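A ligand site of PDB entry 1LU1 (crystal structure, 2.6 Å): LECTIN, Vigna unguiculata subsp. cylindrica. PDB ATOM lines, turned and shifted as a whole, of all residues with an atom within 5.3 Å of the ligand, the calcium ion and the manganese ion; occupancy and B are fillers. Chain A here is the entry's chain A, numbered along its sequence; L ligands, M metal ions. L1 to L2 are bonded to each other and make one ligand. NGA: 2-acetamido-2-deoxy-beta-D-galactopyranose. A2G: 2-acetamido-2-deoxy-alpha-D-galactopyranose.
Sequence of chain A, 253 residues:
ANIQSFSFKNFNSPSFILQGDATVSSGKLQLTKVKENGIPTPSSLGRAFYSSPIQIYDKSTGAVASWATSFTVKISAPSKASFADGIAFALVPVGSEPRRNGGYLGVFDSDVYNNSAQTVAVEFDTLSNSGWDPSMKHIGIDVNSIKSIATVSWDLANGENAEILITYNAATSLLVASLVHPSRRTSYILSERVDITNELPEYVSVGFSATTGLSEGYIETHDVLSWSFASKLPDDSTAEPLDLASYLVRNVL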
ATOM      1  N   ALA A  84       2.712  10.609 -11.917  1.00  0.00           N
ATOM      2  CA  ALA A  84       1.438  11.299 -12.135  1.00  0.00           C
ATOM      3  C   ALA A  84       0.672  10.477 -13.171  1.00  0.00           C
ATOM      4  O   ALA A  84       1.287   9.924 -14.093  1.00  0.00           O
ATOM      5  CB  ALA A  84       1.670  12.697 -12.646  1.00  0.00           C
ATOM      6  N   ASP A  85      -0.646  10.374 -13.041  1.00  0.00           N
ATOM      7  CA  ASP A  85      -1.415  10.978 -11.962  1.00  0.00           C
ATOM      8  C   ASP A  85      -2.047   9.951 -11.040  1.00  0.00           C
ATOM      9  O   ASP A  85      -2.402  10.259  -9.914  1.00  0.00           O
ATOM     10  CB  ASP A  85      -2.521  11.868 -12.544  1.00  0.00           C
ATOM     11  CG  ASP A  85      -2.243  13.346 -12.350  1.00  0.00           C
ATOM     12  OD1 ASP A  85      -2.221  13.787 -11.187  1.00  0.00           O
ATOM     13  OD2 ASP A  85      -2.049  14.046 -13.370  1.00  0.00           O
ATOM     14  N   ASN A 101      -9.543  15.116 -17.058  1.00  0.00           N
ATOM     15  CA  ASN A 101      -8.272  14.394 -17.067  1.00  0.00           C
ATOM     16  C   ASN A 101      -7.336  14.916 -15.973  1.00  0.00           C
ATOM     17  O   ASN A 101      -7.755  15.665 -15.091  1.00  0.00           O
ATOM     18  CB  ASN A 101      -7.586  14.493 -18.434  1.00  0.00           C
ATOM     19  CG  ASN A 101      -7.363  15.949 -18.903  1.00  0.00           C
ATOM     20  OD1 ASN A 101      -6.708  16.182 -19.910  1.00  0.00           O
ATOM     21  ND2 ASN A 101      -7.916  16.890 -18.162  1.00  0.00           N
ATOM     22  N   GLY A 102      -6.071  14.514 -16.020  1.00  0.00           N
ATOM     23  CA  GLY A 102      -5.132  14.962 -15.010  1.00  0.00           C
ATOM     24  C   GLY A 102      -5.436  14.442 -13.615  1.00  0.00           C
ATOM     25  O   GLY A 102      -5.714  13.251 -13.431  1.00  0.00           O
ATOM     26  N   GLY A 103      -5.397  15.338 -12.641  1.00  0.00           N
ATOM     27  CA  GLY A 103      -5.647  14.965 -11.256  1.00  0.00           C
ATOM     28  C   GLY A 103      -7.044  14.490 -10.937  1.00  0.00           C
ATOM     29  O   GLY A 103      -7.328  14.142  -9.785  1.00  0.00           O
ATOM     30  N   TYR A 104      -7.926  14.482 -11.923  1.00  0.00           N
ATOM     31  CA  TYR A 104      -9.299  14.023 -11.697  1.00  0.00           C
ATOM     32  C   TYR A 104      -9.433  12.550 -12.064  1.00  0.00           C
ATOM     33  O   TYR A 104     -10.505  11.956 -11.939  1.00  0.00           O
ATOM     34  CB  TYR A 104     -10.283  14.887 -12.500  1.00  0.00           C
ATOM     35  CG  TYR A 104     -10.413  16.276 -11.924  1.00  0.00           C
ATOM     36  CD1 TYR A 104     -11.255  16.518 -10.848  1.00  0.00           C
ATOM     37  CD2 TYR A 104      -9.648  17.337 -12.424  1.00  0.00           C
ATOM     38  CE1 TYR A 104     -11.349  17.777 -10.265  1.00  0.00           C
ATOM     39  CE2 TYR A 104      -9.738  18.613 -11.855  1.00  0.00           C
ATOM     40  CZ  TYR A 104     -10.592  18.828 -10.772  1.00  0.00           C
ATOM     41  OH  TYR A 104     -10.682  20.073 -10.203  1.00  0.00           O
ATOM     42  N   GLU A 123      -8.963   5.187  -5.161  1.00  0.00           N
ATOM     43  CA  GLU A 123      -7.856   5.685  -5.950  1.00  0.00           C
ATOM     44  C   GLU A 123      -6.499   5.408  -5.363  1.00  0.00           C
ATOM     45  O   GLU A 123      -6.322   5.320  -4.141  1.00  0.00           O
ATOM     46  CB  GLU A 123      -7.974   7.187  -6.133  1.00  0.00           C
ATOM     47  CG  GLU A 123      -8.129   7.896  -4.815  1.00  0.00           C
ATOM     48  CD  GLU A 123      -7.667   9.325  -4.855  1.00  0.00           C
ATOM     49  OE1 GLU A 123      -8.438  10.199  -5.314  1.00  0.00           O
ATOM     50  OE2 GLU A 123      -6.521   9.581  -4.433  1.00  0.00           O
ATOM     51  N   ASP A 125      -3.525   7.389  -5.878  1.00  0.00           N
ATOM     52  CA  ASP A 125      -3.028   8.702  -6.250  1.00  0.00           C
ATOM     53  C   ASP A 125      -1.508   8.847  -6.171  1.00  0.00           C
ATOM     54  O   ASP A 125      -0.962   8.849  -5.074  1.00  0.00           O
ATOM     55  CB  ASP A 125      -3.675   9.708  -5.318  1.00  0.00           C
ATOM     56  CG  ASP A 125      -3.831  11.059  -5.937  1.00  0.00           C
ATOM     57  OD1 ASP A 125      -3.009  11.396  -6.820  1.00  0.00           O
ATOM     58  OD2 ASP A 125      -4.758  11.785  -5.522  1.00  0.00           O
ATOM     59  N   LEU A 127       0.234  11.560  -7.313  1.00  0.00           N
ATOM     60  CA  LEU A 127       0.627  12.972  -7.360  1.00  0.00           C
ATOM     61  C   LEU A 127      -0.299  13.805  -6.480  1.00  0.00           C
ATOM     62  O   LEU A 127      -1.525  13.816  -6.656  1.00  0.00           O
ATOM     63  CB  LEU A 127       0.594  13.515  -8.786  1.00  0.00           C
ATOM     64  CG  LEU A 127       0.996  14.991  -8.890  1.00  0.00           C
ATOM     65  CD1 LEU A 127       2.435  15.097  -9.368  1.00  0.00           C
ATOM     66  CD2 LEU A 127       0.069  15.717  -9.826  1.00  0.00           C
ATOM     67  N   SER A 128       0.303  14.517  -5.532  1.00  0.00           N
ATOM     68  CA  SER A 128      -0.439  15.340  -4.597  1.00  0.00           C
ATOM     69  C   SER A 128      -0.894  16.668  -5.205  1.00  0.00           C
ATOM     70  O   SER A 128      -0.082  17.507  -5.563  1.00  0.00           O
ATOM     71  CB  SER A 128       0.427  15.614  -3.373  1.00  0.00           C
ATOM     72  OG  SER A 128      -0.374  16.042  -2.292  1.00  0.00           O
ATOM     73  N   ASN A 129      -2.213  16.856  -5.297  1.00  0.00           N
ATOM     74  CA  ASN A 129      -2.762  18.092  -5.832  1.00  0.00           C
ATOM     75  C   ASN A 129      -3.116  19.001  -4.656  1.00  0.00           C
ATOM     76  O   ASN A 129      -4.093  18.765  -3.949  1.00  0.00           O
ATOM     77  CB  ASN A 129      -4.021  17.810  -6.649  1.00  0.00           C
ATOM     78  CG  ASN A 129      -3.770  16.835  -7.781  1.00  0.00           C
ATOM     79  OD1 ASN A 129      -4.082  15.647  -7.667  1.00  0.00           O
ATOM     80  ND2 ASN A 129      -3.220  17.331  -8.875  1.00  0.00           N
ATOM     81  N   SER A 130      -2.313  20.041  -4.456  1.00  0.00           N
ATOM     82  CA  SER A 130      -2.475  21.002  -3.367  1.00  0.00           C
ATOM     83  C   SER A 130      -3.897  21.358  -2.915  1.00  0.00           C
ATOM     84  O   SER A 130      -4.118  21.617  -1.726  1.00  0.00           O
ATOM     85  CB  SER A 130      -1.748  22.297  -3.720  1.00  0.00           C
ATOM     86  OG  SER A 130      -1.456  22.341  -5.103  1.00  0.00           O
ATOM     87  N   TRP A 132      -6.720  19.444  -2.728  1.00  0.00           N
ATOM     88  CA  TRP A 132      -7.533  18.442  -2.030  1.00  0.00           C
ATOM     89  C   TRP A 132      -6.769  17.191  -1.624  1.00  0.00           C
ATOM     90  O   TRP A 132      -7.338  16.305  -1.000  1.00  0.00           O
ATOM     91  CB  TRP A 132      -8.686  18.002  -2.931  1.00  0.00           C
ATOM     92  CG  TRP A 132      -8.193  17.389  -4.218  1.00  0.00           C
ATOM     93  CD1 TRP A 132      -7.634  16.153  -4.376  1.00  0.00           C
ATOM     94  CD2 TRP A 132      -8.203  17.994  -5.511  1.00  0.00           C
ATOM     95  NE1 TRP A 132      -7.275  15.950  -5.687  1.00  0.00           N
ATOM     96  CE2 TRP A 132      -7.626  17.067  -6.414  1.00  0.00           C
ATOM     97  CE3 TRP A 132      -8.646  19.230  -6.012  1.00  0.00           C
ATOM     98  CZ2 TRP A 132      -7.466  17.334  -7.769  1.00  0.00           C
ATOM     99  CZ3 TRP A 132      -8.487  19.503  -7.360  1.00  0.00           C
ATOM    100  CH2 TRP A 132      -7.912  18.554  -8.228  1.00  0.00           C
ATOM    101  N   ASP A 133      -5.491  17.130  -1.964  1.00  0.00           N
ATOM    102  CA  ASP A 133      -4.697  15.941  -1.666  1.00  0.00           C
ATOM    103  C   ASP A 133      -3.826  16.022  -0.425  1.00  0.00           C
ATOM    104  O   ASP A 133      -3.372  17.098  -0.031  1.00  0.00           O
ATOM    105  CB  ASP A 133      -3.788  15.625  -2.862  1.00  0.00           C
ATOM    106  CG  ASP A 133      -4.412  14.644  -3.828  1.00  0.00           C
ATOM    107  OD1 ASP A 133      -5.491  14.108  -3.491  1.00  0.00           O
ATOM    108  OD2 ASP A 133      -3.829  14.416  -4.915  1.00  0.00           O
ATOM    109  N   PRO A 134      -3.580  14.867   0.205  1.00  0.00           N
ATOM    110  CA  PRO A 134      -2.738  14.787   1.405  1.00  0.00           C
ATOM    111  C   PRO A 134      -1.296  15.008   0.975  1.00  0.00           C
ATOM    112  O   PRO A 134      -1.008  14.982  -0.216  1.00  0.00           O
ATOM    113  CB  PRO A 134      -2.958  13.356   1.909  1.00  0.00           C
ATOM    114  CG  PRO A 134      -4.133  12.833   1.136  1.00  0.00           C
ATOM    115  CD  PRO A 134      -4.119  13.551  -0.158  1.00  0.00           C
ATOM    116  N   HIS A 138      -0.824   8.352  -1.966  1.00  0.00           N
ATOM    117  CA  HIS A 138      -1.795   7.715  -1.100  1.00  0.00           C
ATOM    118  C   HIS A 138      -2.879   6.880  -1.772  1.00  0.00           C
ATOM    119  O   HIS A 138      -3.076   6.932  -2.979  1.00  0.00           O
ATOM    120  CB  HIS A 138      -2.496   8.807  -0.324  1.00  0.00           C
ATOM    121  CG  HIS A 138      -3.113   9.859  -1.203  1.00  0.00           C
ATOM    122  ND1 HIS A 138      -2.384  10.802  -1.886  1.00  0.00           N
ATOM    123  CD2 HIS A 138      -4.399  10.035  -1.585  1.00  0.00           C
ATOM    124  CE1 HIS A 138      -3.231  11.519  -2.646  1.00  0.00           C
ATOM    125  NE2 HIS A 138      -4.470  11.099  -2.500  1.00  0.00           N
ATOM    126  N   ASP A 142     -12.925   7.644  -2.619  1.00  0.00           N
ATOM    127  CA  ASP A 142     -13.637   8.800  -3.158  1.00  0.00           C
ATOM    128  C   ASP A 142     -15.121   8.547  -3.364  1.00  0.00           C
ATOM    129  O   ASP A 142     -15.499   7.631  -4.086  1.00  0.00           O
ATOM    130  CB  ASP A 142     -13.033   9.224  -4.492  1.00  0.00           C
ATOM    131  CG  ASP A 142     -11.542   9.449  -4.413  1.00  0.00           C
ATOM    132  OD1 ASP A 142     -11.045   9.772  -3.312  1.00  0.00           O
ATOM    133  OD2 ASP A 142     -10.864   9.285  -5.445  1.00  0.00           O
ATOM    134  N   ILE A 146     -13.379  14.274  -5.929  1.00  0.00           N
ATOM    135  CA  ILE A 146     -11.988  13.841  -6.019  1.00  0.00           C
ATOM    136  C   ILE A 146     -11.259  13.999  -4.672  1.00  0.00           C
ATOM    137  O   ILE A 146     -10.110  13.572  -4.519  1.00  0.00           O
ATOM    138  CB  ILE A 146     -11.232  14.596  -7.139  1.00  0.00           C
ATOM    139  CG1 ILE A 146      -9.921  13.871  -7.459  1.00  0.00           C
ATOM    140  CG2 ILE A 146     -10.970  16.040  -6.731  1.00  0.00           C
ATOM    141  CD1 ILE A 146     -10.104  12.521  -8.158  1.00  0.00           C
ATOM    142  N   SER A 148     -10.833  12.660  -1.390  1.00  0.00           N
ATOM    143  CA  SER A 148     -11.128  11.420  -0.682  1.00  0.00           C
ATOM    144  C   SER A 148     -11.697  11.654   0.716  1.00  0.00           C
ATOM    145  O   SER A 148     -11.341  12.630   1.374  1.00  0.00           O
ATOM    146  CB  SER A 148      -9.836  10.586  -0.591  1.00  0.00           C
ATOM    147  OG  SER A 148      -9.039  10.740  -1.747  1.00  0.00           O
ATOM    148  N   THR A 212      -2.374  10.263 -16.887  1.00  0.00           N
ATOM    149  CA  THR A 212      -0.994  10.660 -16.667  1.00  0.00           C
ATOM    150  C   THR A 212      -1.009  12.184 -16.540  1.00  0.00           C
ATOM    151  O   THR A 212      -2.023  12.823 -16.852  1.00  0.00           O
ATOM    152  CB  THR A 212      -0.094  10.221 -17.834  1.00  0.00           C
ATOM    153  OG1 THR A 212      -0.627  10.686 -19.077  1.00  0.00           O
ATOM    154  CG2 THR A 212       0.011   8.713 -17.878  1.00  0.00           C
ATOM    155  N   GLY A 213       0.092  12.754 -16.064  1.00  0.00           N
ATOM    156  CA  GLY A 213       0.181  14.196 -15.852  1.00  0.00           C
ATOM    157  C   GLY A 213       0.133  15.064 -17.083  1.00  0.00           C
ATOM    158  O   GLY A 213       0.453  14.617 -18.186  1.00  0.00           O
ATOM    159  N   LEU A 214      -0.252  16.317 -16.900  1.00  0.00           N
ATOM    160  CA  LEU A 214      -0.382  17.270 -17.996  1.00  0.00           C
ATOM    161  C   LEU A 214       0.909  17.985 -18.351  1.00  0.00           C
ATOM    162  O   LEU A 214       0.897  18.951 -19.110  1.00  0.00           O
ATOM    163  CB  LEU A 214      -1.458  18.295 -17.660  1.00  0.00           C
ATOM    164  CG  LEU A 214      -2.819  17.721 -17.278  1.00  0.00           C
ATOM    165  CD1 LEU A 214      -3.780  18.868 -16.951  1.00  0.00           C
ATOM    166  CD2 LEU A 214      -3.369  16.884 -18.430  1.00  0.00           C
ATOM    167  N   SER A 215       2.023  17.525 -17.794  1.00  0.00           N
ATOM    168  CA  SER A 215       3.329  18.140 -18.064  1.00  0.00           C
ATOM    169  C   SER A 215       4.282  17.153 -18.688  1.00  0.00           C
ATOM    170  O   SER A 215       4.111  15.954 -18.562  1.00  0.00           O
ATOM    171  CB  SER A 215       3.937  18.698 -16.782  1.00  0.00           C
ATOM    172  OG  SER A 215       3.118  19.724 -16.266  1.00  0.00           O
ATOM    173  N   TYR A 218       5.740  14.509 -16.029  1.00  0.00           N
ATOM    174  CA  TYR A 218       4.919  13.843 -15.044  1.00  0.00           C
ATOM    175  C   TYR A 218       4.179  12.695 -15.689  1.00  0.00           C
ATOM    176  O   TYR A 218       3.012  12.830 -16.051  1.00  0.00           O
ATOM    177  CB  TYR A 218       3.948  14.824 -14.433  1.00  0.00           C
ATOM    178  CG  TYR A 218       4.646  15.801 -13.539  1.00  0.00           C
ATOM    179  CD1 TYR A 218       5.273  16.918 -14.066  1.00  0.00           C
ATOM    180  CD2 TYR A 218       4.672  15.607 -12.165  1.00  0.00           C
ATOM    181  CE1 TYR A 218       5.905  17.842 -13.241  1.00  0.00           C
ATOM    182  CE2 TYR A 218       5.296  16.521 -11.333  1.00  0.00           C
ATOM    183  CZ  TYR A 218       5.902  17.638 -11.867  1.00  0.00           C
ATOM    184  OH  TYR A 218       6.482  18.559 -11.027  1.00  0.00           O
HETATM  185  C1  NGA L   1       0.769  23.690 -11.508  1.00  0.00           C
HETATM  186  C2  NGA L   1       0.205  22.286 -11.339  1.00  0.00           C
HETATM  187  C3  NGA L   1      -0.605  21.912 -12.549  1.00  0.00           C
HETATM  188  C4  NGA L   1      -1.610  22.973 -12.979  1.00  0.00           C
HETATM  189  C5  NGA L   1      -0.944  24.331 -13.042  1.00  0.00           C
HETATM  190  C6  NGA L   1      -1.915  25.480 -13.359  1.00  0.00           C
HETATM  191  C7  NGA L   1       1.278  20.556 -10.091  1.00  0.00           C
HETATM  192  C8  NGA L   1       2.442  19.602  -9.969  1.00  0.00           C
HETATM  193  N2  NGA L   1       1.285  21.332 -11.160  1.00  0.00           N
HETATM  194  O1  NGA L   1       1.319  24.077 -10.295  1.00  0.00           O
HETATM  195  O3  NGA L   1      -1.327  20.692 -12.267  1.00  0.00           O
HETATM  196  O4  NGA L   1      -2.683  22.960 -12.046  1.00  0.00           O
HETATM  197  O5  NGA L   1      -0.296  24.596 -11.779  1.00  0.00           O
HETATM  198  O7  NGA L   1       0.343  20.568  -9.253  1.00  0.00           O
HETATM  199  O5  A2G L   2      -0.355  19.212 -13.948  1.00  0.00           O
HETATM  200  C1  A2G L   2      -1.547  19.792 -13.367  1.00  0.00           C
HETATM  201  C2  A2G L   2      -2.551  18.684 -12.983  1.00  0.00           C
HETATM  202  N2  A2G L   2      -3.668  19.269 -12.268  1.00  0.00           N
HETATM  203  C3  A2G L   2      -1.901  17.598 -12.118  1.00  0.00           C
HETATM  204  O3  A2G L   2      -2.849  16.569 -11.849  1.00  0.00           O
HETATM  205  C4  A2G L   2      -0.675  17.036 -12.849  1.00  0.00           C
HETATM  206  O4  A2G L   2      -1.102  16.475 -14.083  1.00  0.00           O
HETATM  207  C5  A2G L   2       0.277  18.172 -13.147  1.00  0.00           C
HETATM  208  C6  A2G L   2       1.507  17.686 -13.921  1.00  0.00           C
HETATM  209  O6  A2G L   2       2.398  18.762 -14.112  1.00  0.00           O
HETATM  210  C7  A2G L   2      -4.923  18.879 -12.539  1.00  0.00           C
HETATM  211  O7  A2G L   2      -5.178  18.057 -13.412  1.00  0.00           O
HETATM  212  C8  A2G L   2      -6.061  19.495 -11.732  1.00  0.00           C
HETATM  213 CA    CA M   1      -3.814  13.607  -7.206  1.00  0.00          CA
HETATM  214 MN    MN M   2      -6.483  11.914  -3.798  1.00  0.00          MN
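The backbone NH (N) of Leu 214 sits at hydrogen-bond distance from an oxygen (O4) of A2G L2 (2.9 Å).
An oxygen (O7) of A2G L2 lies within hydrogen-bond range of the backbone NH (N) of Gly 103, at 2.8 Å.
OD2 of Asp 85 is in hydrogen-bond range of O4 of A2G L2, 2.7 Å away.
The side-chain amide nitrogen (ND2) of Asn 129 lies within hydrogen-bond range of an oxygen (O3) of A2G L2, 3.1 Å away.
The side-chain hydroxyl of Ser 215 lies within hydrogen-bond range of an oxygen (O6) of A2G L2 (2.5 Å).
OD1 of Asp 133 sits close to NE1 of Trp 132, 3.4 Å away.
The side-chain carboxylate (OD2) of Asp 142 sits close to the side-chain carboxylate (OE1) of Glu 123, 2.6 Å away.
OG of Ser 148 lies within hydrogen-bond range of OD1 of Asp 142 (2.7 Å).
The backbone carbonyl oxygen of Tyr 218 is in hydrogen-bond range of the backbone NH of Gly 213 (2.9 Å).
Residues that only touch the ligand: Gly 213 (3.2 Å), Tyr 218 (3.4 Å), Gly 102 (3.5 Å), Tyr 104 (3.8 Å) and Asn 101 (3.9 Å).
Hydrophobic or aromatic side chains within 4 Å of the ligand: Tyr 104, Leu 127, Leu 214 and Tyr 218.
Within 4 Å of the ligand: Asp 85, Asn 101, Gly 102, Gly 103, Tyr 104, Leu 127, Asn 129, Gly 213, Leu 214, Ser 215 and Tyr 218.
The nearest printed residue that does not touch the ligand is Trp 132 (4.1 Å).
Four residues have an atom within 4 Å of the calcium ion: Asp 125, Leu 127, Asn 129 and Asp 133.
Ser 148 touches the manganese ion.
Within 4 Å of the manganese ion: Glu 123, Asp 125, Asp 133, His 138 and Ser 148.
Along chain A the residues within 4 Å of the manganese ion span positions 123 to 148.
The nearest printed residue that does not touch the manganese ion is Ile 146 (4.1 Å).
OD1 of Asn 129 is bound to the calcium ion (2.1 Å).
O of Leu 127 is bound to the calcium ion.
OD1 of Asp 125 binds the calcium ion (2.4 Å).
OD2 of Asp 133 binds the calcium ion.
OD2 of Asp 125 is bound to the calcium ion (2.7 Å).
The manganese ion is bound by OE2 of Glu 123 (2.4 Å), OD1 of Asp 133 (2.4 Å), OD2 of Asp 125 (2.4 Å) and NE2 of His 138 (2.5 Å).
The manganese ion has four donor atoms within binding distance.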
